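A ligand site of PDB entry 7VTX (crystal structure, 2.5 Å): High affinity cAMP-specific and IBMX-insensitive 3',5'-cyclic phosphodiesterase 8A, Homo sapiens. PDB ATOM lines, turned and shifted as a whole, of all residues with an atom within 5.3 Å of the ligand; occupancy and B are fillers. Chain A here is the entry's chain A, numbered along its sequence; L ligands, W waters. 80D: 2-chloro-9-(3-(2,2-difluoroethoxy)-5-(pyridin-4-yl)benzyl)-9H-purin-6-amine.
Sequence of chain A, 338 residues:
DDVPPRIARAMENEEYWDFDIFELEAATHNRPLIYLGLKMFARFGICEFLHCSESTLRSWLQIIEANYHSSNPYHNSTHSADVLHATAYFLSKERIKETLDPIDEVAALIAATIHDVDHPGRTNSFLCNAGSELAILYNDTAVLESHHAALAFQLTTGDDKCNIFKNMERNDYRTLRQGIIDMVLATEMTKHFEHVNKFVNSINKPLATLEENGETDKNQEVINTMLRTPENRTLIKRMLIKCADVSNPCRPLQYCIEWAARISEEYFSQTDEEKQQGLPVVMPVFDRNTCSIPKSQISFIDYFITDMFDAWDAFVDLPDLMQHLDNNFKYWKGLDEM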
ATOM      1  N   TYR A  74      21.248 -11.168 -20.808  1.00  0.00           N
ATOM      2  CA  TYR A  74      21.285  -9.948 -19.986  1.00  0.00           C
ATOM      3  C   TYR A  74      20.241  -9.981 -18.868  1.00  0.00           C
ATOM      4  O   TYR A  74      20.595  -9.857 -17.687  1.00  0.00           O
ATOM      5  CB  TYR A  74      21.070  -8.719 -20.867  1.00  0.00           C
ATOM      6  CG  TYR A  74      21.133  -7.384 -20.159  1.00  0.00           C
ATOM      7  CD1 TYR A  74      22.334  -6.698 -20.018  1.00  0.00           C
ATOM      8  CD2 TYR A  74      19.972  -6.790 -19.660  1.00  0.00           C
ATOM      9  CE1 TYR A  74      22.394  -5.451 -19.390  1.00  0.00           C
ATOM     10  CE2 TYR A  74      20.019  -5.551 -19.024  1.00  0.00           C
ATOM     11  CZ  TYR A  74      21.229  -4.887 -18.888  1.00  0.00           C
ATOM     12  OH  TYR A  74      21.268  -3.670 -18.272  1.00  0.00           O
ATOM     13  N   THR A 187      10.270   2.083 -14.979  1.00  0.00           N
ATOM     14  CA  THR A 187      11.347   1.562 -15.833  1.00  0.00           C
ATOM     15  C   THR A 187      10.955   1.349 -17.318  1.00  0.00           C
ATOM     16  O   THR A 187      11.822   1.051 -18.138  1.00  0.00           O
ATOM     17  CB  THR A 187      11.878   0.216 -15.296  1.00  0.00           C
ATOM     18  OG1 THR A 187      10.838  -0.761 -15.316  1.00  0.00           O
ATOM     19  CG2 THR A 187      12.424   0.382 -13.878  1.00  0.00           C
ATOM     20  N   GLU A 188       9.674   1.493 -17.656  1.00  0.00           N
ATOM     21  CA  GLU A 188       9.228   1.348 -19.047  1.00  0.00           C
ATOM     22  C   GLU A 188       9.910   2.371 -19.955  1.00  0.00           C
ATOM     23  O   GLU A 188       9.856   3.571 -19.692  1.00  0.00           O
ATOM     24  CB  GLU A 188       7.694   1.466 -19.163  1.00  0.00           C
ATOM     25  CG  GLU A 188       7.165   1.049 -20.535  1.00  0.00           C
ATOM     26  CD  GLU A 188       5.671   1.248 -20.706  1.00  0.00           C
ATOM     27  OE1 GLU A 188       5.033   1.888 -19.835  1.00  0.00           O
ATOM     28  OE2 GLU A 188       5.126   0.790 -21.726  1.00  0.00           O
ATOM     29  N   MET A 189      10.532   1.884 -21.023  1.00  0.00           N
ATOM     30  CA  MET A 189      11.329   2.698 -21.943  1.00  0.00           C
ATOM     31  C   MET A 189      10.560   3.874 -22.554  1.00  0.00           C
ATOM     32  O   MET A 189      11.115   4.963 -22.714  1.00  0.00           O
ATOM     33  CB  MET A 189      11.970   1.793 -23.014  1.00  0.00           C
ATOM     34  CG  MET A 189      12.616   2.464 -24.220  1.00  0.00           C
ATOM     35  SD  MET A 189      11.474   2.505 -25.627  1.00  0.00           S
ATOM     36  CE  MET A 189      12.558   2.922 -26.993  1.00  0.00           C
ATOM     37  N   HIS A 192      10.618   7.456 -20.757  1.00  0.00           N
ATOM     38  CA  HIS A 192      11.941   7.990 -20.387  1.00  0.00           C
ATOM     39  C   HIS A 192      11.966   9.516 -20.297  1.00  0.00           C
ATOM     40  O   HIS A 192      12.256  10.081 -19.237  1.00  0.00           O
ATOM     41  CB  HIS A 192      13.009   7.506 -21.381  1.00  0.00           C
ATOM     42  CG  HIS A 192      14.361   8.147 -21.195  1.00  0.00           C
ATOM     43  ND1 HIS A 192      15.327   7.630 -20.365  1.00  0.00           N
ATOM     44  CD2 HIS A 192      14.885   9.270 -21.735  1.00  0.00           C
ATOM     45  CE1 HIS A 192      16.399   8.404 -20.404  1.00  0.00           C
ATOM     46  NE2 HIS A 192      16.158   9.410 -21.220  1.00  0.00           N
ATOM     47  N   LYS A 242      15.495   4.448 -12.467  1.00  0.00           N
ATOM     48  CA  LYS A 242      15.822   4.578 -13.890  1.00  0.00           C
ATOM     49  C   LYS A 242      17.323   4.586 -14.146  1.00  0.00           C
ATOM     50  O   LYS A 242      17.803   3.920 -15.064  1.00  0.00           O
ATOM     51  CB  LYS A 242      15.216   5.856 -14.493  1.00  0.00           C
ATOM     52  CG  LYS A 242      13.753   5.702 -14.889  1.00  0.00           C
ATOM     53  CD  LYS A 242      13.213   6.951 -15.579  1.00  0.00           C
ATOM     54  CE  LYS A 242      13.837   7.182 -16.947  1.00  0.00           C
ATOM     55  NZ  LYS A 242      13.837   5.964 -17.803  1.00  0.00           N
ATOM     56  N   ASP A 245      18.809   1.088 -13.192  1.00  0.00           N
ATOM     57  CA  ASP A 245      18.479   0.107 -14.214  1.00  0.00           C
ATOM     58  C   ASP A 245      19.476   0.090 -15.376  1.00  0.00           C
ATOM     59  O   ASP A 245      19.843  -0.990 -15.850  1.00  0.00           O
ATOM     60  CB  ASP A 245      17.065   0.314 -14.771  1.00  0.00           C
ATOM     61  CG  ASP A 245      16.649  -0.793 -15.742  1.00  0.00           C
ATOM     62  OD1 ASP A 245      16.771  -1.975 -15.378  1.00  0.00           O
ATOM     63  OD2 ASP A 245      16.226  -0.487 -16.871  1.00  0.00           O
ATOM     64  N   VAL A 246      19.898   1.274 -15.841  1.00  0.00           N
ATOM     65  CA  VAL A 246      20.839   1.391 -16.958  1.00  0.00           C
ATOM     66  C   VAL A 246      22.176   2.038 -16.550  1.00  0.00           C
ATOM     67  O   VAL A 246      22.715   2.878 -17.255  1.00  0.00           O
ATOM     68  CB  VAL A 246      20.188   2.122 -18.166  1.00  0.00           C
ATOM     69  CG1 VAL A 246      19.001   1.323 -18.680  1.00  0.00           C
ATOM     70  CG2 VAL A 246      19.739   3.533 -17.823  1.00  0.00           C
ATOM     71  N   ASN A 248      25.007   0.403 -16.312  1.00  0.00           N
ATOM     72  CA  ASN A 248      26.125  -0.357 -16.890  1.00  0.00           C
ATOM     73  C   ASN A 248      27.166   0.471 -17.692  1.00  0.00           C
ATOM     74  O   ASN A 248      28.373   0.203 -17.557  1.00  0.00           O
ATOM     75  CB  ASN A 248      25.672  -1.630 -17.661  1.00  0.00           C
ATOM     76  CG  ASN A 248      24.745  -1.338 -18.844  1.00  0.00           C
ATOM     77  OD1 ASN A 248      25.210  -1.019 -19.946  1.00  0.00           O
ATOM     78  ND2 ASN A 248      23.453  -1.498 -18.630  1.00  0.00           N
ATOM     79  N   PRO A 249      26.722   1.475 -18.475  1.00  0.00           N
ATOM     80  CA  PRO A 249      27.735   2.311 -19.139  1.00  0.00           C
ATOM     81  C   PRO A 249      28.565   3.201 -18.193  1.00  0.00           C
ATOM     82  O   PRO A 249      29.593   3.735 -18.631  1.00  0.00           O
ATOM     83  CB  PRO A 249      26.893   3.163 -20.103  1.00  0.00           C
ATOM     84  CG  PRO A 249      25.568   2.489 -20.187  1.00  0.00           C
ATOM     85  CD  PRO A 249      25.375   1.951 -18.818  1.00  0.00           C
ATOM     86  N   TRP A 259      28.409  -6.099 -20.117  1.00  0.00           N
ATOM     87  CA  TRP A 259      26.979  -5.744 -20.173  1.00  0.00           C
ATOM     88  C   TRP A 259      26.493  -5.410 -21.584  1.00  0.00           C
ATOM     89  O   TRP A 259      25.373  -5.776 -21.957  1.00  0.00           O
ATOM     90  CB  TRP A 259      26.657  -4.578 -19.228  1.00  0.00           C
ATOM     91  CG  TRP A 259      26.614  -4.951 -17.760  1.00  0.00           C
ATOM     92  CD1 TRP A 259      27.338  -4.386 -16.760  1.00  0.00           C
ATOM     93  CD2 TRP A 259      25.799  -5.959 -17.147  1.00  0.00           C
ATOM     94  NE1 TRP A 259      27.029  -4.967 -15.552  1.00  0.00           N
ATOM     95  CE2 TRP A 259      26.089  -5.936 -15.759  1.00  0.00           C
ATOM     96  CE3 TRP A 259      24.848  -6.874 -17.620  1.00  0.00           C
ATOM     97  CZ2 TRP A 259      25.465  -6.815 -14.860  1.00  0.00           C
ATOM     98  CZ3 TRP A 259      24.236  -7.734 -16.721  1.00  0.00           C
ATOM     99  CH2 TRP A 259      24.542  -7.696 -15.353  1.00  0.00           C
ATOM    100  N   ALA A 260      27.328  -4.726 -22.355  1.00  0.00           N
ATOM    101  CA  ALA A 260      27.026  -4.415 -23.769  1.00  0.00           C
ATOM    102  C   ALA A 260      26.901  -5.668 -24.634  1.00  0.00           C
ATOM    103  O   ALA A 260      26.063  -5.731 -25.527  1.00  0.00           O
ATOM    104  CB  ALA A 260      28.082  -3.484 -24.346  1.00  0.00           C
ATOM    105  N   ILE A 263      23.372  -7.615 -23.466  1.00  0.00           N
ATOM    106  CA  ILE A 263      22.188  -6.938 -24.009  1.00  0.00           C
ATOM    107  C   ILE A 263      22.132  -6.975 -25.545  1.00  0.00           C
ATOM    108  O   ILE A 263      21.050  -7.155 -26.110  1.00  0.00           O
ATOM    109  CB  ILE A 263      22.056  -5.477 -23.488  1.00  0.00           C
ATOM    110  CG1 ILE A 263      20.684  -4.879 -23.852  1.00  0.00           C
ATOM    111  CG2 ILE A 263      23.161  -4.567 -24.012  1.00  0.00           C
ATOM    112  CD1 ILE A 263      19.485  -5.658 -23.354  1.00  0.00           C
ATOM    113  N   TYR A 267      19.257  -8.860 -28.017  1.00  0.00           N
ATOM    114  CA  TYR A 267      18.582  -8.208 -29.147  1.00  0.00           C
ATOM    115  C   TYR A 267      18.857  -8.866 -30.507  1.00  0.00           C
ATOM    116  O   TYR A 267      18.002  -8.795 -31.400  1.00  0.00           O
ATOM    117  CB  TYR A 267      18.914  -6.706 -29.210  1.00  0.00           C
ATOM    118  CG  TYR A 267      18.392  -5.867 -28.055  1.00  0.00           C
ATOM    119  CD1 TYR A 267      19.099  -4.750 -27.594  1.00  0.00           C
ATOM    120  CD2 TYR A 267      17.181  -6.184 -27.415  1.00  0.00           C
ATOM    121  CE1 TYR A 267      18.611  -3.977 -26.538  1.00  0.00           C
ATOM    122  CE2 TYR A 267      16.701  -5.422 -26.355  1.00  0.00           C
ATOM    123  CZ  TYR A 267      17.421  -4.330 -25.919  1.00  0.00           C
ATOM    124  OH  TYR A 267      16.913  -3.597 -24.882  1.00  0.00           O
ATOM    125  N   MET A 283      13.808  -3.591 -33.953  1.00  0.00           N
ATOM    126  CA  MET A 283      15.194  -3.132 -33.829  1.00  0.00           C
ATOM    127  C   MET A 283      15.985  -3.655 -35.035  1.00  0.00           C
ATOM    128  O   MET A 283      16.667  -4.681 -34.922  1.00  0.00           O
ATOM    129  CB  MET A 283      15.808  -3.647 -32.534  1.00  0.00           C
ATOM    130  CG  MET A 283      15.302  -2.962 -31.284  1.00  0.00           C
ATOM    131  SD  MET A 283      15.931  -3.730 -29.788  1.00  0.00           S
ATOM    132  CE  MET A 283      15.385  -2.555 -28.549  1.00  0.00           C
ATOM    133  N   PHE A 286      19.973  -3.790 -34.587  1.00  0.00           N
ATOM    134  CA  PHE A 286      20.484  -4.865 -33.720  1.00  0.00           C
ATOM    135  C   PHE A 286      20.294  -6.256 -34.333  1.00  0.00           C
ATOM    136  O   PHE A 286      19.480  -7.057 -33.871  1.00  0.00           O
ATOM    137  CB  PHE A 286      19.856  -4.778 -32.323  1.00  0.00           C
ATOM    138  CG  PHE A 286      20.273  -3.561 -31.551  1.00  0.00           C
ATOM    139  CD1 PHE A 286      19.551  -2.376 -31.641  1.00  0.00           C
ATOM    140  CD2 PHE A 286      21.404  -3.593 -30.733  1.00  0.00           C
ATOM    141  CE1 PHE A 286      19.941  -1.253 -30.933  1.00  0.00           C
ATOM    142  CE2 PHE A 286      21.804  -2.472 -30.023  1.00  0.00           C
ATOM    143  CZ  PHE A 286      21.073  -1.297 -30.124  1.00  0.00           C
ATOM    144  N   SER A 296      26.763   1.235 -31.724  1.00  0.00           N
ATOM    145  CA  SER A 296      25.442   1.113 -31.100  1.00  0.00           C
ATOM    146  C   SER A 296      25.425   1.529 -29.617  1.00  0.00           C
ATOM    147  O   SER A 296      24.412   2.042 -29.131  1.00  0.00           O
ATOM    148  CB  SER A 296      24.915  -0.317 -31.249  1.00  0.00           C
ATOM    149  OG  SER A 296      24.730  -0.653 -32.606  1.00  0.00           O
ATOM    150  N   GLN A 297      26.526   1.285 -28.911  1.00  0.00           N
ATOM    151  CA  GLN A 297      26.701   1.757 -27.532  1.00  0.00           C
ATOM    152  C   GLN A 297      26.861   3.286 -27.447  1.00  0.00           C
ATOM    153  O   GLN A 297      26.290   3.921 -26.552  1.00  0.00           O
ATOM    154  CB  GLN A 297      27.898   1.071 -26.862  1.00  0.00           C
ATOM    155  CG  GLN A 297      27.698  -0.403 -26.573  1.00  0.00           C
ATOM    156  CD  GLN A 297      26.486  -0.664 -25.704  1.00  0.00           C
ATOM    157  OE1 GLN A 297      26.207   0.100 -24.770  1.00  0.00           O
ATOM    158  NE2 GLN A 297      25.739  -1.728 -25.995  1.00  0.00           N
ATOM    159  N   PHE A 300      23.460   4.629 -28.054  1.00  0.00           N
ATOM    160  CA  PHE A 300      22.688   4.360 -26.832  1.00  0.00           C
ATOM    161  C   PHE A 300      23.019   5.390 -25.734  1.00  0.00           C
ATOM    162  O   PHE A 300      22.114   5.936 -25.107  1.00  0.00           O
ATOM    163  CB  PHE A 300      22.941   2.923 -26.337  1.00  0.00           C
ATOM    164  CG  PHE A 300      22.288   2.599 -25.023  1.00  0.00           C
ATOM    165  CD1 PHE A 300      20.922   2.342 -24.945  1.00  0.00           C
ATOM    166  CD2 PHE A 300      23.037   2.561 -23.847  1.00  0.00           C
ATOM    167  CE1 PHE A 300      20.314   2.063 -23.731  1.00  0.00           C
ATOM    168  CE2 PHE A 300      22.438   2.271 -22.630  1.00  0.00           C
ATOM    169  CZ  PHE A 300      21.075   2.023 -22.562  1.00  0.00           C
ATOM    170  N   PHE A 304      19.951   8.252 -24.464  1.00  0.00           N
ATOM    171  CA  PHE A 304      19.354   8.014 -23.131  1.00  0.00           C
ATOM    172  C   PHE A 304      20.248   8.416 -21.944  1.00  0.00           C
ATOM    173  O   PHE A 304      19.767   9.045 -20.990  1.00  0.00           O
ATOM    174  CB  PHE A 304      19.023   6.523 -22.967  1.00  0.00           C
ATOM    175  CG  PHE A 304      18.053   5.995 -23.998  1.00  0.00           C
ATOM    176  CD1 PHE A 304      18.511   5.359 -25.140  1.00  0.00           C
ATOM    177  CD2 PHE A 304      16.683   6.126 -23.807  1.00  0.00           C
ATOM    178  CE1 PHE A 304      17.620   4.871 -26.090  1.00  0.00           C
ATOM    179  CE2 PHE A 304      15.781   5.640 -24.749  1.00  0.00           C
ATOM    180  CZ  PHE A 304      16.259   5.012 -25.888  1.00  0.00           C
HETATM  181  N1  80D L   1      22.785  -0.893 -24.590  1.00  0.00           N
HETATM  182  C8  80D L   1      20.444  -1.570 -20.895  1.00  0.00           C
HETATM  183  C5  80D L   1      21.864  -1.224 -22.433  1.00  0.00           C
HETATM  184  C6  80D L   1      22.983  -0.976 -23.257  1.00  0.00           C
HETATM  185  N3  80D L   1      20.414  -1.252 -24.373  1.00  0.00           N
HETATM  186  C4  80D L   1      20.638  -1.331 -23.056  1.00  0.00           C
HETATM  187  C2  80D L   1      21.539  -1.029 -25.038  1.00  0.00           C
HETATM  188  N7  80D L   1      19.730  -1.555 -22.051  1.00  0.00           N
HETATM  189  N9  80D L   1      21.731  -1.374 -21.063  1.00  0.00           N
HETATM  190  N10 80D L   1      24.221  -0.808 -22.804  1.00  0.00           N
HETATM  191 CL1  80D L   1      21.364  -0.888 -26.754  1.00  0.00          CL
HETATM  192  C12 80D L   1      18.288  -1.737 -22.213  1.00  0.00           C
HETATM  193  C13 80D L   1      17.589  -0.500 -22.737  1.00  0.00           C
HETATM  194  C14 80D L   1      17.172   0.498 -21.861  1.00  0.00           C
HETATM  195  C15 80D L   1      16.628   1.666 -22.376  1.00  0.00           C
HETATM  196  C16 80D L   1      16.489   1.860 -23.743  1.00  0.00           C
HETATM  197  C17 80D L   1      16.888   0.862 -24.633  1.00  0.00           C
HETATM  198  C18 80D L   1      17.427  -0.324 -24.106  1.00  0.00           C
HETATM  199  O19 80D L   1      16.165   2.804 -21.753  1.00  0.00           O
HETATM  200  C20 80D L   1      16.231   2.931 -20.320  1.00  0.00           C
HETATM  201  C21 80D L   1      14.739   3.217 -19.957  1.00  0.00           C
HETATM  202  F22 80D L   1      14.233   4.198 -20.749  1.00  0.00           F
HETATM  203  F23 80D L   1      13.988   2.109 -20.202  1.00  0.00           F
HETATM  204  C24 80D L   1      16.821   1.057 -26.100  1.00  0.00           C
HETATM  205  C25 80D L   1      15.785   1.771 -26.691  1.00  0.00           C
HETATM  206  C26 80D L   1      15.768   1.949 -28.063  1.00  0.00           C
HETATM  207  N27 80D L   1      16.708   1.471 -28.877  1.00  0.00           N
HETATM  208  C28 80D L   1      17.712   0.788 -28.316  1.00  0.00           C
HETATM  209  C29 80D L   1      17.809   0.568 -26.954  1.00  0.00           C
HETATM  210  O   HOH W   1      14.425   1.861 -16.922  1.00  0.00           O
HETATM  211  O   HOH W   2      18.614  -2.180 -18.148  1.00  0.00           O
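OE1 of Gln 297 is in hydrogen-bond range of N10 of the ligand (2.9 Å). The side-chain amide nitrogen (ND2) of Asn 248 lies within hydrogen-bond range of a nitrogen (N9) of the ligand, at 3.0 Å.
The side-chain amide nitrogen (ND2) of Asn 248 sits at hydrogen-bond distance from the side-chain hydroxyl (OH) of Tyr 74. ND1 of His 192 sits at hydrogen-bond distance from NZ of Lys 242 (3.4 Å).
The backbone carbonyl oxygen (O) of Thr 187 sits close to a fluorine (F23) of the ligand (3.2 Å). The side-chain amino group of Lys 242 lies close to a fluorine (F22) of the ligand (3.5 Å). Merely in contact with the ligand: Tyr 74, Met 189, His 192, Val 246, Ile 263, Tyr 267, Phe 286, Phe 300 and Phe 304. Hydrophobic or aromatic side chains that line the ligand: Tyr 74, Met 189, His 192, Val 246, Ile 263, Tyr 267, Phe 286, Phe 300 and Phe 304. Of the 20 residues printed, 13 come within 4 Å of the ligand.
Water W1 lies within hydrogen-bond range of the side-chain carboxylate (OD2) of Asp 245 (3.0 Å) and the backbone carbonyl oxygen (O) of Thr 187 (3.0 Å). Water W2 lies within hydrogen-bond range of O of Asp 245 (2.9 Å) and OH of Tyr 74 (3.0 Å).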
